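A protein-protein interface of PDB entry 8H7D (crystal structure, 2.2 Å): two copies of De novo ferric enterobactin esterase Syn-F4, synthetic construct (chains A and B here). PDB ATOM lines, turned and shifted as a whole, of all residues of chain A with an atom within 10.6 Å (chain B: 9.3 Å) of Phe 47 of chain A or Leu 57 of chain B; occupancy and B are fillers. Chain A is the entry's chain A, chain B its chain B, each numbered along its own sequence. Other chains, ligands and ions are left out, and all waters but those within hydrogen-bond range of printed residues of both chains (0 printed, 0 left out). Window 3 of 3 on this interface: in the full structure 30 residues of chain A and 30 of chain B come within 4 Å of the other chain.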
ATOM      1  N   GLN A  39      10.565   7.819  -9.655  1.00  0.00           N
ATOM      2  CA  GLN A  39      10.333   6.369  -9.866  1.00  0.00           C
ATOM      3  C   GLN A  39       8.938   6.153 -10.401  1.00  0.00           C
ATOM      4  O   GLN A  39       8.708   5.287 -11.243  1.00  0.00           O
ATOM      5  CB  GLN A  39      10.465   5.556  -8.567  1.00  0.00           C
ATOM      6  CG  GLN A  39      11.742   5.759  -7.778  1.00  0.00           C
ATOM      7  CD  GLN A  39      12.712   4.617  -7.916  1.00  0.00           C
ATOM      8  OE1 GLN A  39      13.092   4.243  -9.044  1.00  0.00           O
ATOM      9  NE2 GLN A  39      13.146   4.057  -6.769  1.00  0.00           N
ATOM     10  N   LEU A  40       8.020   6.948  -9.868  1.00  0.00           N
ATOM     11  CA  LEU A  40       6.632   6.953 -10.273  1.00  0.00           C
ATOM     12  C   LEU A  40       6.496   7.402 -11.739  1.00  0.00           C
ATOM     13  O   LEU A  40       6.028   6.633 -12.576  1.00  0.00           O
ATOM     14  CB  LEU A  40       5.829   7.823  -9.302  1.00  0.00           C
ATOM     15  CG  LEU A  40       4.379   8.173  -9.621  1.00  0.00           C
ATOM     16  CD1 LEU A  40       3.618   6.963 -10.096  1.00  0.00           C
ATOM     17  CD2 LEU A  40       3.684   8.763  -8.402  1.00  0.00           C
ATOM     18  N   VAL A  41       6.936   8.618 -12.049  1.00  0.00           N
ATOM     19  CA  VAL A  41       7.004   9.095 -13.441  1.00  0.00           C
ATOM     20  C   VAL A  41       7.573   8.014 -14.372  1.00  0.00           C
ATOM     21  O   VAL A  41       6.980   7.700 -15.413  1.00  0.00           O
ATOM     22  CB  VAL A  41       7.856  10.388 -13.554  1.00  0.00           C
ATOM     23  CG1 VAL A  41       8.543  10.549 -14.918  1.00  0.00           C
ATOM     24  CG2 VAL A  41       6.996  11.605 -13.287  1.00  0.00           C
ATOM     25  N   LYS A  42       8.724   7.467 -13.981  1.00  0.00           N
ATOM     26  CA  LYS A  42       9.415   6.431 -14.764  1.00  0.00           C
ATOM     27  C   LYS A  42       8.609   5.134 -14.904  1.00  0.00           C
ATOM     28  O   LYS A  42       8.663   4.501 -15.960  1.00  0.00           O
ATOM     29  CB  LYS A  42      10.811   6.129 -14.195  1.00  0.00           C
ATOM     30  CG  LYS A  42      11.900   7.093 -14.630  1.00  0.00           C
ATOM     31  CD  LYS A  42      12.116   7.055 -16.133  1.00  0.00           C
ATOM     32  CE  LYS A  42      13.202   8.000 -16.599  1.00  0.00           C
ATOM     33  NZ  LYS A  42      13.363   7.907 -18.082  1.00  0.00           N
ATOM     34  N   HIS A  43       7.881   4.751 -13.848  1.00  0.00           N
ATOM     35  CA  HIS A  43       6.953   3.617 -13.894  1.00  0.00           C
ATOM     36  C   HIS A  43       5.839   3.863 -14.909  1.00  0.00           C
ATOM     37  O   HIS A  43       5.658   3.081 -15.845  1.00  0.00           O
ATOM     38  CB  HIS A  43       6.348   3.346 -12.506  1.00  0.00           C
ATOM     39  CG  HIS A  43       5.456   2.144 -12.458  1.00  0.00           C
ATOM     40  ND1 HIS A  43       4.336   2.075 -11.657  1.00  0.00           N
ATOM     41  CD2 HIS A  43       5.508   0.970 -13.133  1.00  0.00           C
ATOM     42  CE1 HIS A  43       3.742   0.906 -11.831  1.00  0.00           C
ATOM     43  NE2 HIS A  43       4.435   0.216 -12.721  1.00  0.00           N
ATOM     44  N   VAL A  44       5.117   4.963 -14.724  1.00  0.00           N
ATOM     45  CA  VAL A  44       3.957   5.285 -15.569  1.00  0.00           C
ATOM     46  C   VAL A  44       4.373   5.432 -17.041  1.00  0.00           C
ATOM     47  O   VAL A  44       3.687   4.934 -17.929  1.00  0.00           O
ATOM     48  CB  VAL A  44       3.217   6.558 -15.133  1.00  0.00           C
ATOM     49  CG1 VAL A  44       1.978   6.765 -15.992  1.00  0.00           C
ATOM     50  CG2 VAL A  44       2.772   6.458 -13.695  1.00  0.00           C
ATOM     51  N   HIS A  45       5.493   6.116 -17.281  1.00  0.00           N
ATOM     52  CA  HIS A  45       6.108   6.238 -18.614  1.00  0.00           C
ATOM     53  C   HIS A  45       6.138   4.877 -19.353  1.00  0.00           C
ATOM     54  O   HIS A  45       5.724   4.768 -20.520  1.00  0.00           O
ATOM     55  CB  HIS A  45       7.527   6.822 -18.459  1.00  0.00           C
ATOM     56  CG  HIS A  45       8.276   7.001 -19.749  1.00  0.00           C
ATOM     57  ND1 HIS A  45       9.228   6.105 -20.187  1.00  0.00           N
ATOM     58  CD2 HIS A  45       8.231   7.983 -20.681  1.00  0.00           C
ATOM     59  CE1 HIS A  45       9.731   6.520 -21.335  1.00  0.00           C
ATOM     60  NE2 HIS A  45       9.140   7.657 -21.659  1.00  0.00           N
ATOM     61  N   HIS A  46       6.618   3.853 -18.647  1.00  0.00           N
ATOM     62  CA  HIS A  46       6.659   2.482 -19.159  1.00  0.00           C
ATOM     63  C   HIS A  46       5.275   1.826 -19.195  1.00  0.00           C
ATOM     64  O   HIS A  46       5.037   0.957 -20.020  1.00  0.00           O
ATOM     65  CB  HIS A  46       7.653   1.632 -18.350  1.00  0.00           C
ATOM     66  CG  HIS A  46       9.078   2.082 -18.474  1.00  0.00           C
ATOM     67  ND1 HIS A  46      10.034   1.805 -17.522  1.00  0.00           N
ATOM     68  CD2 HIS A  46       9.707   2.796 -19.436  1.00  0.00           C
ATOM     69  CE1 HIS A  46      11.191   2.326 -17.892  1.00  0.00           C
ATOM     70  NE2 HIS A  46      11.020   2.933 -19.051  1.00  0.00           N
ATOM     71  N   PHE A  47       4.383   2.233 -18.294  1.00  0.00           N
ATOM     72  CA  PHE A  47       2.962   1.833 -18.331  1.00  0.00           C
ATOM     73  C   PHE A  47       2.178   2.358 -19.552  1.00  0.00           C
ATOM     74  O   PHE A  47       1.382   1.627 -20.147  1.00  0.00           O
ATOM     75  CB  PHE A  47       2.261   2.263 -17.029  1.00  0.00           C
ATOM     76  CG  PHE A  47       0.758   2.310 -17.127  1.00  0.00           C
ATOM     77  CD1 PHE A  47       0.006   1.149 -16.996  1.00  0.00           C
ATOM     78  CD2 PHE A  47       0.093   3.517 -17.367  1.00  0.00           C
ATOM     79  CE1 PHE A  47      -1.382   1.181 -17.098  1.00  0.00           C
ATOM     80  CE2 PHE A  47      -1.290   3.558 -17.470  1.00  0.00           C
ATOM     81  CZ  PHE A  47      -2.030   2.387 -17.333  1.00  0.00           C
ATOM     82  N   MET A  48       2.375   3.631 -19.889  1.00  0.00           N
ATOM     83  CA  MET A  48       1.664   4.278 -21.001  1.00  0.00           C
ATOM     84  C   MET A  48       2.248   3.897 -22.363  1.00  0.00           C
ATOM     85  O   MET A  48       2.656   2.759 -22.591  1.00  0.00           O
ATOM     86  CB  MET A  48       1.697   5.796 -20.842  1.00  0.00           C
ATOM     87  CG  MET A  48       3.069   6.407 -21.060  1.00  0.00           C
ATOM     88  SD  MET A  48       3.051   8.150 -20.704  1.00  0.00           S
ATOM     89  CE  MET A  48       4.378   8.761 -21.742  1.00  0.00           C
ATOM     90  N   LEU A  57      -5.295  10.815 -21.326  1.00  0.00           N
ATOM     91  CA  LEU A  57      -4.649   9.505 -21.332  1.00  0.00           C
ATOM     92  C   LEU A  57      -3.204   9.599 -20.791  1.00  0.00           C
ATOM     93  O   LEU A  57      -2.935   9.291 -19.625  1.00  0.00           O
ATOM     94  CB  LEU A  57      -4.702   8.918 -22.757  1.00  0.00           C
ATOM     95  CG  LEU A  57      -4.067   7.539 -23.000  1.00  0.00           C
ATOM     96  CD1 LEU A  57      -5.112   6.446 -22.837  1.00  0.00           C
ATOM     97  CD2 LEU A  57      -3.413   7.447 -24.373  1.00  0.00           C
ATOM     98  N   GLN A  58      -2.304  10.061 -21.655  1.00  0.00           N
ATOM     99  CA  GLN A  58      -0.870  10.170 -21.396  1.00  0.00           C
ATOM    100  C   GLN A  58      -0.508  11.650 -21.094  1.00  0.00           C
ATOM    101  O   GLN A  58       0.664  12.020 -20.931  1.00  0.00           O
ATOM    102  CB  GLN A  58      -0.150   9.588 -22.626  1.00  0.00           C
ATOM    103  CG  GLN A  58       1.353   9.755 -22.710  1.00  0.00           C
ATOM    104  CD  GLN A  58       1.815  10.803 -23.711  1.00  0.00           C
ATOM    105  OE1 GLN A  58       1.197  11.860 -23.859  1.00  0.00           O
ATOM    106  NE2 GLN A  58       2.924  10.517 -24.397  1.00  0.00           N
ATOM    107  N   ASP A  59      -1.548  12.478 -20.973  1.00  0.00           N
ATOM    108  CA  ASP A  59      -1.447  13.877 -20.556  1.00  0.00           C
ATOM    109  C   ASP A  59      -0.938  13.983 -19.104  1.00  0.00           C
ATOM    110  O   ASP A  59      -0.538  15.066 -18.645  1.00  0.00           O
ATOM    111  CB  ASP A  59      -2.845  14.523 -20.679  1.00  0.00           C
ATOM    112  CG  ASP A  59      -2.808  16.009 -21.015  1.00  0.00           C
ATOM    113  OD1 ASP A  59      -1.780  16.689 -20.810  1.00  0.00           O
ATOM    114  OD2 ASP A  59      -3.845  16.506 -21.494  1.00  0.00           O
ATOM    115  N   ILE A  60      -0.983  12.852 -18.390  1.00  0.00           N
ATOM    116  CA  ILE A  60      -0.698  12.783 -16.970  1.00  0.00           C
ATOM    117  C   ILE A  60       0.790  12.615 -16.684  1.00  0.00           C
ATOM    118  O   ILE A  60       1.284  13.171 -15.707  1.00  0.00           O
ATOM    119  CB  ILE A  60      -1.543  11.662 -16.320  1.00  0.00           C
ATOM    120  CG1 ILE A  60      -3.001  12.141 -16.188  1.00  0.00           C
ATOM    121  CG2 ILE A  60      -1.013  11.268 -14.941  1.00  0.00           C
ATOM    122  CD1 ILE A  60      -4.017  11.038 -15.968  1.00  0.00           C
ATOM    123  N   VAL A  61       1.481  11.834 -17.514  1.00  0.00           N
ATOM    124  CA  VAL A  61       2.937  11.686 -17.417  1.00  0.00           C
ATOM    125  C   VAL A  61       3.664  12.984 -17.742  1.00  0.00           C
ATOM    126  O   VAL A  61       4.708  13.261 -17.147  1.00  0.00           O
ATOM    127  CB  VAL A  61       3.479  10.522 -18.289  1.00  0.00           C
ATOM    128  CG1 VAL A  61       4.829  10.822 -18.961  1.00  0.00           C
ATOM    129  CG2 VAL A  61       3.600   9.279 -17.431  1.00  0.00           C
ATOM    130  N   LEU A  64       3.114  14.873 -14.749  1.00  0.00           N
ATOM    131  CA  LEU A  64       3.923  14.208 -13.726  1.00  0.00           C
ATOM    132  C   LEU A  64       5.431  14.546 -13.860  1.00  0.00           C
ATOM    133  O   LEU A  64       6.081  14.913 -12.877  1.00  0.00           O
ATOM    134  CB  LEU A  64       3.670  12.690 -13.716  1.00  0.00           C
ATOM    135  CG  LEU A  64       2.585  12.136 -12.785  1.00  0.00           C
ATOM    136  CD1 LEU A  64       2.520  10.620 -12.892  1.00  0.00           C
ATOM    137  CD2 LEU A  64       2.822  12.501 -11.328  1.00  0.00           C
ATOM    138  N   LEU B  40      -4.162  16.669  -9.784  1.00  0.00           N
ATOM    139  CA  LEU B  40      -3.788  15.472 -10.510  1.00  0.00           C
ATOM    140  C   LEU B  40      -4.262  14.183  -9.809  1.00  0.00           C
ATOM    141  O   LEU B  40      -4.463  13.168 -10.465  1.00  0.00           O
ATOM    142  CB  LEU B  40      -2.263  15.491 -10.687  1.00  0.00           C
ATOM    143  CG  LEU B  40      -1.526  14.392 -11.447  1.00  0.00           C
ATOM    144  CD1 LEU B  40      -1.723  14.537 -12.942  1.00  0.00           C
ATOM    145  CD2 LEU B  40      -0.041  14.435 -11.112  1.00  0.00           C
ATOM    146  N   VAL B  41      -4.431  14.227  -8.485  1.00  0.00           N
ATOM    147  CA  VAL B  41      -5.025  13.110  -7.713  1.00  0.00           C
ATOM    148  C   VAL B  41      -6.546  13.033  -7.948  1.00  0.00           C
ATOM    149  O   VAL B  41      -7.086  11.953  -8.171  1.00  0.00           O
ATOM    150  CB  VAL B  41      -4.711  13.246  -6.191  1.00  0.00           C
ATOM    151  CG1 VAL B  41      -5.710  12.487  -5.315  1.00  0.00           C
ATOM    152  CG2 VAL B  41      -3.294  12.785  -5.895  1.00  0.00           C
ATOM    153  N   HIS B  43      -7.968  14.355 -10.582  1.00  0.00           N
ATOM    154  CA  HIS B  43      -8.044  14.084 -12.032  1.00  0.00           C
ATOM    155  C   HIS B  43      -7.949  12.593 -12.336  1.00  0.00           C
ATOM    156  O   HIS B  43      -8.816  12.037 -13.012  1.00  0.00           O
ATOM    157  CB  HIS B  43      -6.917  14.832 -12.780  1.00  0.00           C
ATOM    158  CG  HIS B  43      -7.220  15.158 -14.213  1.00  0.00           C
ATOM    159  ND1 HIS B  43      -8.266  14.598 -14.918  1.00  0.00           N
ATOM    160  CD2 HIS B  43      -6.585  15.984 -15.079  1.00  0.00           C
ATOM    161  CE1 HIS B  43      -8.270  15.077 -16.149  1.00  0.00           C
ATOM    162  NE2 HIS B  43      -7.259  15.919 -16.273  1.00  0.00           N
ATOM    163  N   VAL B  44      -6.906  11.951 -11.818  1.00  0.00           N
ATOM    164  CA  VAL B  44      -6.705  10.504 -11.994  1.00  0.00           C
ATOM    165  C   VAL B  44      -7.915   9.719 -11.438  1.00  0.00           C
ATOM    166  O   VAL B  44      -8.356   8.729 -12.029  1.00  0.00           O
ATOM    167  CB  VAL B  44      -5.368  10.039 -11.356  1.00  0.00           C
ATOM    168  CG1 VAL B  44      -5.234   8.522 -11.356  1.00  0.00           C
ATOM    169  CG2 VAL B  44      -4.186  10.620 -12.106  1.00  0.00           C
ATOM    170  N   HIS B  45      -8.458  10.195 -10.321  1.00  0.00           N
ATOM    171  CA  HIS B  45      -9.659   9.610  -9.694  1.00  0.00           C
ATOM    172  C   HIS B  45     -10.937   9.763 -10.579  1.00  0.00           C
ATOM    173  O   HIS B  45     -11.863   8.959 -10.467  1.00  0.00           O
ATOM    174  CB  HIS B  45      -9.837  10.237  -8.290  1.00  0.00           C
ATOM    175  CG  HIS B  45     -10.621   9.405  -7.315  1.00  0.00           C
ATOM    176  ND1 HIS B  45     -11.211   9.949  -6.192  1.00  0.00           N
ATOM    177  CD2 HIS B  45     -10.902   8.080  -7.279  1.00  0.00           C
ATOM    178  CE1 HIS B  45     -11.827   8.999  -5.513  1.00  0.00           C
ATOM    179  NE2 HIS B  45     -11.659   7.857  -6.153  1.00  0.00           N
ATOM    180  N   HIS B  46     -10.964  10.790 -11.439  1.00  0.00           N
ATOM    181  CA  HIS B  46     -12.052  11.021 -12.429  1.00  0.00           C
ATOM    182  C   HIS B  46     -11.958  10.115 -13.677  1.00  0.00           C
ATOM    183  O   HIS B  46     -12.970   9.821 -14.316  1.00  0.00           O
ATOM    184  CB  HIS B  46     -12.090  12.501 -12.880  1.00  0.00           C
ATOM    185  CG  HIS B  46     -12.900  13.399 -11.990  1.00  0.00           C
ATOM    186  ND1 HIS B  46     -12.485  13.780 -10.730  1.00  0.00           N
ATOM    187  CD2 HIS B  46     -14.088  14.015 -12.195  1.00  0.00           C
ATOM    188  CE1 HIS B  46     -13.388  14.581 -10.193  1.00  0.00           C
ATOM    189  NE2 HIS B  46     -14.371  14.738 -11.061  1.00  0.00           N
ATOM    190  N   PHE B  47     -10.741   9.687 -14.003  1.00  0.00           N
ATOM    191  CA  PHE B  47     -10.437   8.895 -15.202  1.00  0.00           C
ATOM    192  C   PHE B  47     -11.006   7.464 -15.201  1.00  0.00           C
ATOM    193  O   PHE B  47     -11.330   6.910 -16.258  1.00  0.00           O
ATOM    194  CB  PHE B  47      -8.910   8.827 -15.341  1.00  0.00           C
ATOM    195  CG  PHE B  47      -8.425   8.417 -16.704  1.00  0.00           C
ATOM    196  CD1 PHE B  47      -8.816   9.125 -17.840  1.00  0.00           C
ATOM    197  CD2 PHE B  47      -7.538   7.350 -16.853  1.00  0.00           C
ATOM    198  CE1 PHE B  47      -8.362   8.759 -19.098  1.00  0.00           C
ATOM    199  CE2 PHE B  47      -7.080   6.981 -18.108  1.00  0.00           C
ATOM    200  CZ  PHE B  47      -7.491   7.687 -19.232  1.00  0.00           C
ATOM    201  N   MET B  48     -11.154   6.893 -14.009  1.00  0.00           N
ATOM    202  CA  MET B  48     -11.365   5.454 -13.842  1.00  0.00           C
ATOM    203  C   MET B  48     -12.836   5.060 -13.973  1.00  0.00           C
ATOM    204  O   MET B  48     -13.145   3.921 -14.325  1.00  0.00           O
ATOM    205  CB  MET B  48     -10.825   5.012 -12.488  1.00  0.00           C
ATOM    206  CG  MET B  48      -9.532   5.703 -12.081  1.00  0.00           C
ATOM    207  SD  MET B  48      -8.545   4.728 -10.942  1.00  0.00           S
ATOM    208  CE  MET B  48      -7.216   5.860 -10.579  1.00  0.00           C
ATOM    209  N   LYS B  56      -5.782  -1.620 -10.908  1.00  0.00           N
ATOM    210  CA  LYS B  56      -5.065  -1.460 -12.166  1.00  0.00           C
ATOM    211  C   LYS B  56      -4.260  -0.145 -12.186  1.00  0.00           C
ATOM    212  O   LYS B  56      -3.028  -0.166 -12.125  1.00  0.00           O
ATOM    213  CB  LYS B  56      -6.064  -1.557 -13.332  1.00  0.00           C
ATOM    214  CG  LYS B  56      -5.459  -1.518 -14.724  1.00  0.00           C
ATOM    215  CD  LYS B  56      -4.663  -2.772 -15.044  1.00  0.00           C
ATOM    216  CE  LYS B  56      -4.022  -2.669 -16.417  1.00  0.00           C
ATOM    217  NZ  LYS B  56      -5.041  -2.653 -17.501  1.00  0.00           N
ATOM    218  N   LEU B  57      -4.968   0.988 -12.235  1.00  0.00           N
ATOM    219  CA  LEU B  57      -4.367   2.334 -12.112  1.00  0.00           C
ATOM    220  C   LEU B  57      -4.393   2.813 -10.647  1.00  0.00           C
ATOM    221  O   LEU B  57      -4.146   3.983 -10.357  1.00  0.00           O
ATOM    222  CB  LEU B  57      -5.126   3.339 -13.002  1.00  0.00           C
ATOM    223  CG  LEU B  57      -4.736   3.440 -14.485  1.00  0.00           C
ATOM    224  CD1 LEU B  57      -5.090   2.177 -15.271  1.00  0.00           C
ATOM    225  CD2 LEU B  57      -5.385   4.673 -15.114  1.00  0.00           C
ATOM    226  N   GLN B  58      -4.673   1.885  -9.736  1.00  0.00           N
ATOM    227  CA  GLN B  58      -4.951   2.178  -8.344  1.00  0.00           C
ATOM    228  C   GLN B  58      -3.653   2.438  -7.582  1.00  0.00           C
ATOM    229  O   GLN B  58      -3.587   3.340  -6.757  1.00  0.00           O
ATOM    230  CB  GLN B  58      -5.734   1.011  -7.720  1.00  0.00           C
ATOM    231  CG  GLN B  58      -6.139   1.188  -6.259  1.00  0.00           C
ATOM    232  CD  GLN B  58      -7.187   2.265  -6.025  1.00  0.00           C
ATOM    233  OE1 GLN B  58      -6.969   3.211  -5.259  1.00  0.00           O
ATOM    234  NE2 GLN B  58      -8.342   2.115  -6.662  1.00  0.00           N
ATOM    235  N   ASP B  59      -2.628   1.632  -7.850  1.00  0.00           N
ATOM    236  CA  ASP B  59      -1.281   1.865  -7.288  1.00  0.00           C
ATOM    237  C   ASP B  59      -0.784   3.298  -7.523  1.00  0.00           C
ATOM    238  O   ASP B  59      -0.166   3.896  -6.653  1.00  0.00           O
ATOM    239  CB  ASP B  59      -0.262   0.860  -7.852  1.00  0.00           C
ATOM    240  CG  ASP B  59      -0.215  -0.442  -7.057  1.00  0.00           C
ATOM    241  OD1 ASP B  59      -0.074  -0.397  -5.814  1.00  0.00           O
ATOM    242  OD2 ASP B  59      -0.311  -1.518  -7.680  1.00  0.00           O
ATOM    243  N   ILE B  60      -1.104   3.840  -8.691  1.00  0.00           N
ATOM    244  CA  ILE B  60      -0.669   5.173  -9.092  1.00  0.00           C
ATOM    245  C   ILE B  60      -1.367   6.253  -8.239  1.00  0.00           C
ATOM    246  O   ILE B  60      -0.692   7.065  -7.606  1.00  0.00           O
ATOM    247  CB  ILE B  60      -0.907   5.439 -10.609  1.00  0.00           C
ATOM    248  CG1 ILE B  60      -0.516   4.238 -11.510  1.00  0.00           C
ATOM    249  CG2 ILE B  60      -0.141   6.670 -11.069  1.00  0.00           C
ATOM    250  CD1 ILE B  60       0.912   3.734 -11.392  1.00  0.00           C
ATOM    251  N   VAL B  61      -2.704   6.250  -8.243  1.00  0.00           N
ATOM    252  CA  VAL B  61      -3.543   7.212  -7.461  1.00  0.00           C
ATOM    253  C   VAL B  61      -3.255   7.183  -5.956  1.00  0.00           C
ATOM    254  O   VAL B  61      -3.248   8.235  -5.319  1.00  0.00           O
ATOM    255  CB  VAL B  61      -5.087   7.018  -7.687  1.00  0.00           C
ATOM    256  CG1 VAL B  61      -5.547   5.613  -7.367  1.00  0.00           C
ATOM    257  CG2 VAL B  61      -5.931   7.972  -6.845  1.00  0.00           C
ATOM    258  N   ASN B  62      -3.080   5.967  -5.420  1.00  0.00           N
ATOM    259  CA  ASN B  62      -2.794   5.708  -4.022  1.00  0.00           C
ATOM    260  C   ASN B  62      -1.469   6.321  -3.652  1.00  0.00           C
ATOM    261  O   ASN B  62      -1.366   6.964  -2.620  1.00  0.00           O
ATOM    262  CB  ASN B  62      -2.704   4.200  -3.747  1.00  0.00           C
ATOM    263  CG  ASN B  62      -4.062   3.529  -3.617  1.00  0.00           C
ATOM    264  OD1 ASN B  62      -5.068   4.160  -3.274  1.00  0.00           O
ATOM    265  ND2 ASN B  62      -4.086   2.222  -3.859  1.00  0.00           N
ATOM    266  N   GLN B  63      -0.478   6.089  -4.507  1.00  0.00           N
ATOM    267  CA  GLN B  63       0.877   6.589  -4.319  1.00  0.00           C
ATOM    268  C   GLN B  63       0.918   8.110  -4.406  1.00  0.00           C
ATOM    269  O   GLN B  63       1.660   8.745  -3.659  1.00  0.00           O
ATOM    270  CB  GLN B  63       1.828   5.975  -5.354  1.00  0.00           C
ATOM    271  CG  GLN B  63       3.312   6.282  -5.144  1.00  0.00           C
ATOM    272  CD  GLN B  63       3.858   5.808  -3.800  1.00  0.00           C
ATOM    273  OE1 GLN B  63       4.405   6.598  -3.025  1.00  0.00           O
ATOM    274  NE2 GLN B  63       3.702   4.518  -3.512  1.00  0.00           N
ATOM    275  N   LEU B  64       0.127   8.688  -5.312  1.00  0.00           N
ATOM    276  CA  LEU B  64       0.027  10.146  -5.416  1.00  0.00           C
ATOM    277  C   LEU B  64      -0.658  10.732  -4.196  1.00  0.00           C
ATOM    278  O   LEU B  64      -0.320  11.816  -3.727  1.00  0.00           O
ATOM    279  CB  LEU B  64      -0.731  10.566  -6.682  1.00  0.00           C
ATOM    280  CG  LEU B  64       0.032  10.399  -7.989  1.00  0.00           C
ATOM    281  CD1 LEU B  64      -0.912  10.659  -9.155  1.00  0.00           C
ATOM    282  CD2 LEU B  64       1.250  11.317  -8.070  1.00  0.00           C
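Of the 16 printed residues of chain A, 7 touch a printed residue of chain B.
Hydrophobic or aromatic side chains of chain A within 4 Å of the printed part of chain B: Leu 40, His 43, Val 44, Phe 47, Ile 60 and Leu 64.
Along chain A the printed residues that touch a printed residue of chain B span positions 40 to 64.
Among the printed residues, 10 pairs touch across the chains.
Among the printed residues, no Asp or Glu carboxylate lies within 4 Å of a Lys or Arg side-chain nitrogen of the other chain.
Leu 40 of chain A touches Ile 60 of chain B, and with the chains exchanged Ile 60 of chain A touches Leu 40 of chain B.
Leu 40 of chain A touches Leu 64 of chain B, and with the chains exchanged Leu 64 of chain A touches Leu 40 of chain B.
Val 44 of chain A touches Ile 60 of chain B, and with the chains exchanged Ile 60 of chain A touches Val 44 of chain B.
Leu 64 of chain A touches its own counterpart, Leu 64 of chain B.
Positions printed for both chains: 40, 41, 43, 44, 45, 46, 47, 48, 57, 58, 59, 60, 61 and 64.
Of the 10 pairs that touch across the chains among the printed residues, 9 have their exchanged pair printed and touching as well.
Among the printed residues, pairs that only touch across the chains: Leu 40 of chain A with Ile 60 of chain B (3.9 Å), Leu 40 of chain A with Leu 64 of chain B (3.5 Å), His 43 of chain A with Ile 60 of chain B (3.8 Å), Val 44 of chain A with Ile 60 of chain B (3.9 Å), Phe 47 of chain A with Leu 57 of chain B (3.7 Å), Leu 57 of chain A with Phe 47 of chain B (3.97 Å), Ile 60 of chain A with Leu 40 of chain B (3.9 Å), Ile 60 of chain A with Val 44 of chain B (3.9 Å), Leu 64 of chain A with Leu 40 of chain B (3.5 Å) and Leu 64 of chain A with Leu 64 of chain B (3.8 Å).
Of chain B, only Leu 57 (3.7 Å) comes within 4 Å of Phe 47 of chain A.
Printed residues of chain A within 4 Å of Leu 57 of chain B: Phe 47 (3.7 Å).
No residue of chain A comes within 4 Å of Lys 56 of chain B.
No residue of chain A comes within 4 Å of Gln 58 of chain B.
Ile 60 of chain B touches just these residues of chain A: Leu 40, His 43 and Val 44.
Of the printed residues of chain B, Leu 40 of chain A touches Ile 60 (3.9 Å) and Leu 64 (3.5 Å).
Of the printed residues of chain A, Leu 40 of chain B touches Ile 60 (3.9 Å) and Leu 64 (3.5 Å).
Printed residues of chain B within 4 Å of His 43 of chain A: Ile 60 (3.8 Å).
Met 48 of chain A touches none of the printed residues of chain B.
The nearest residue of chain B that does not touch Phe 47 of chain A is Lys 56 of chain B (4.7 Å).
The nearest residue of chain A that does not touch Leu 57 of chain B is Ile 60 of chain A (6.6 Å).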
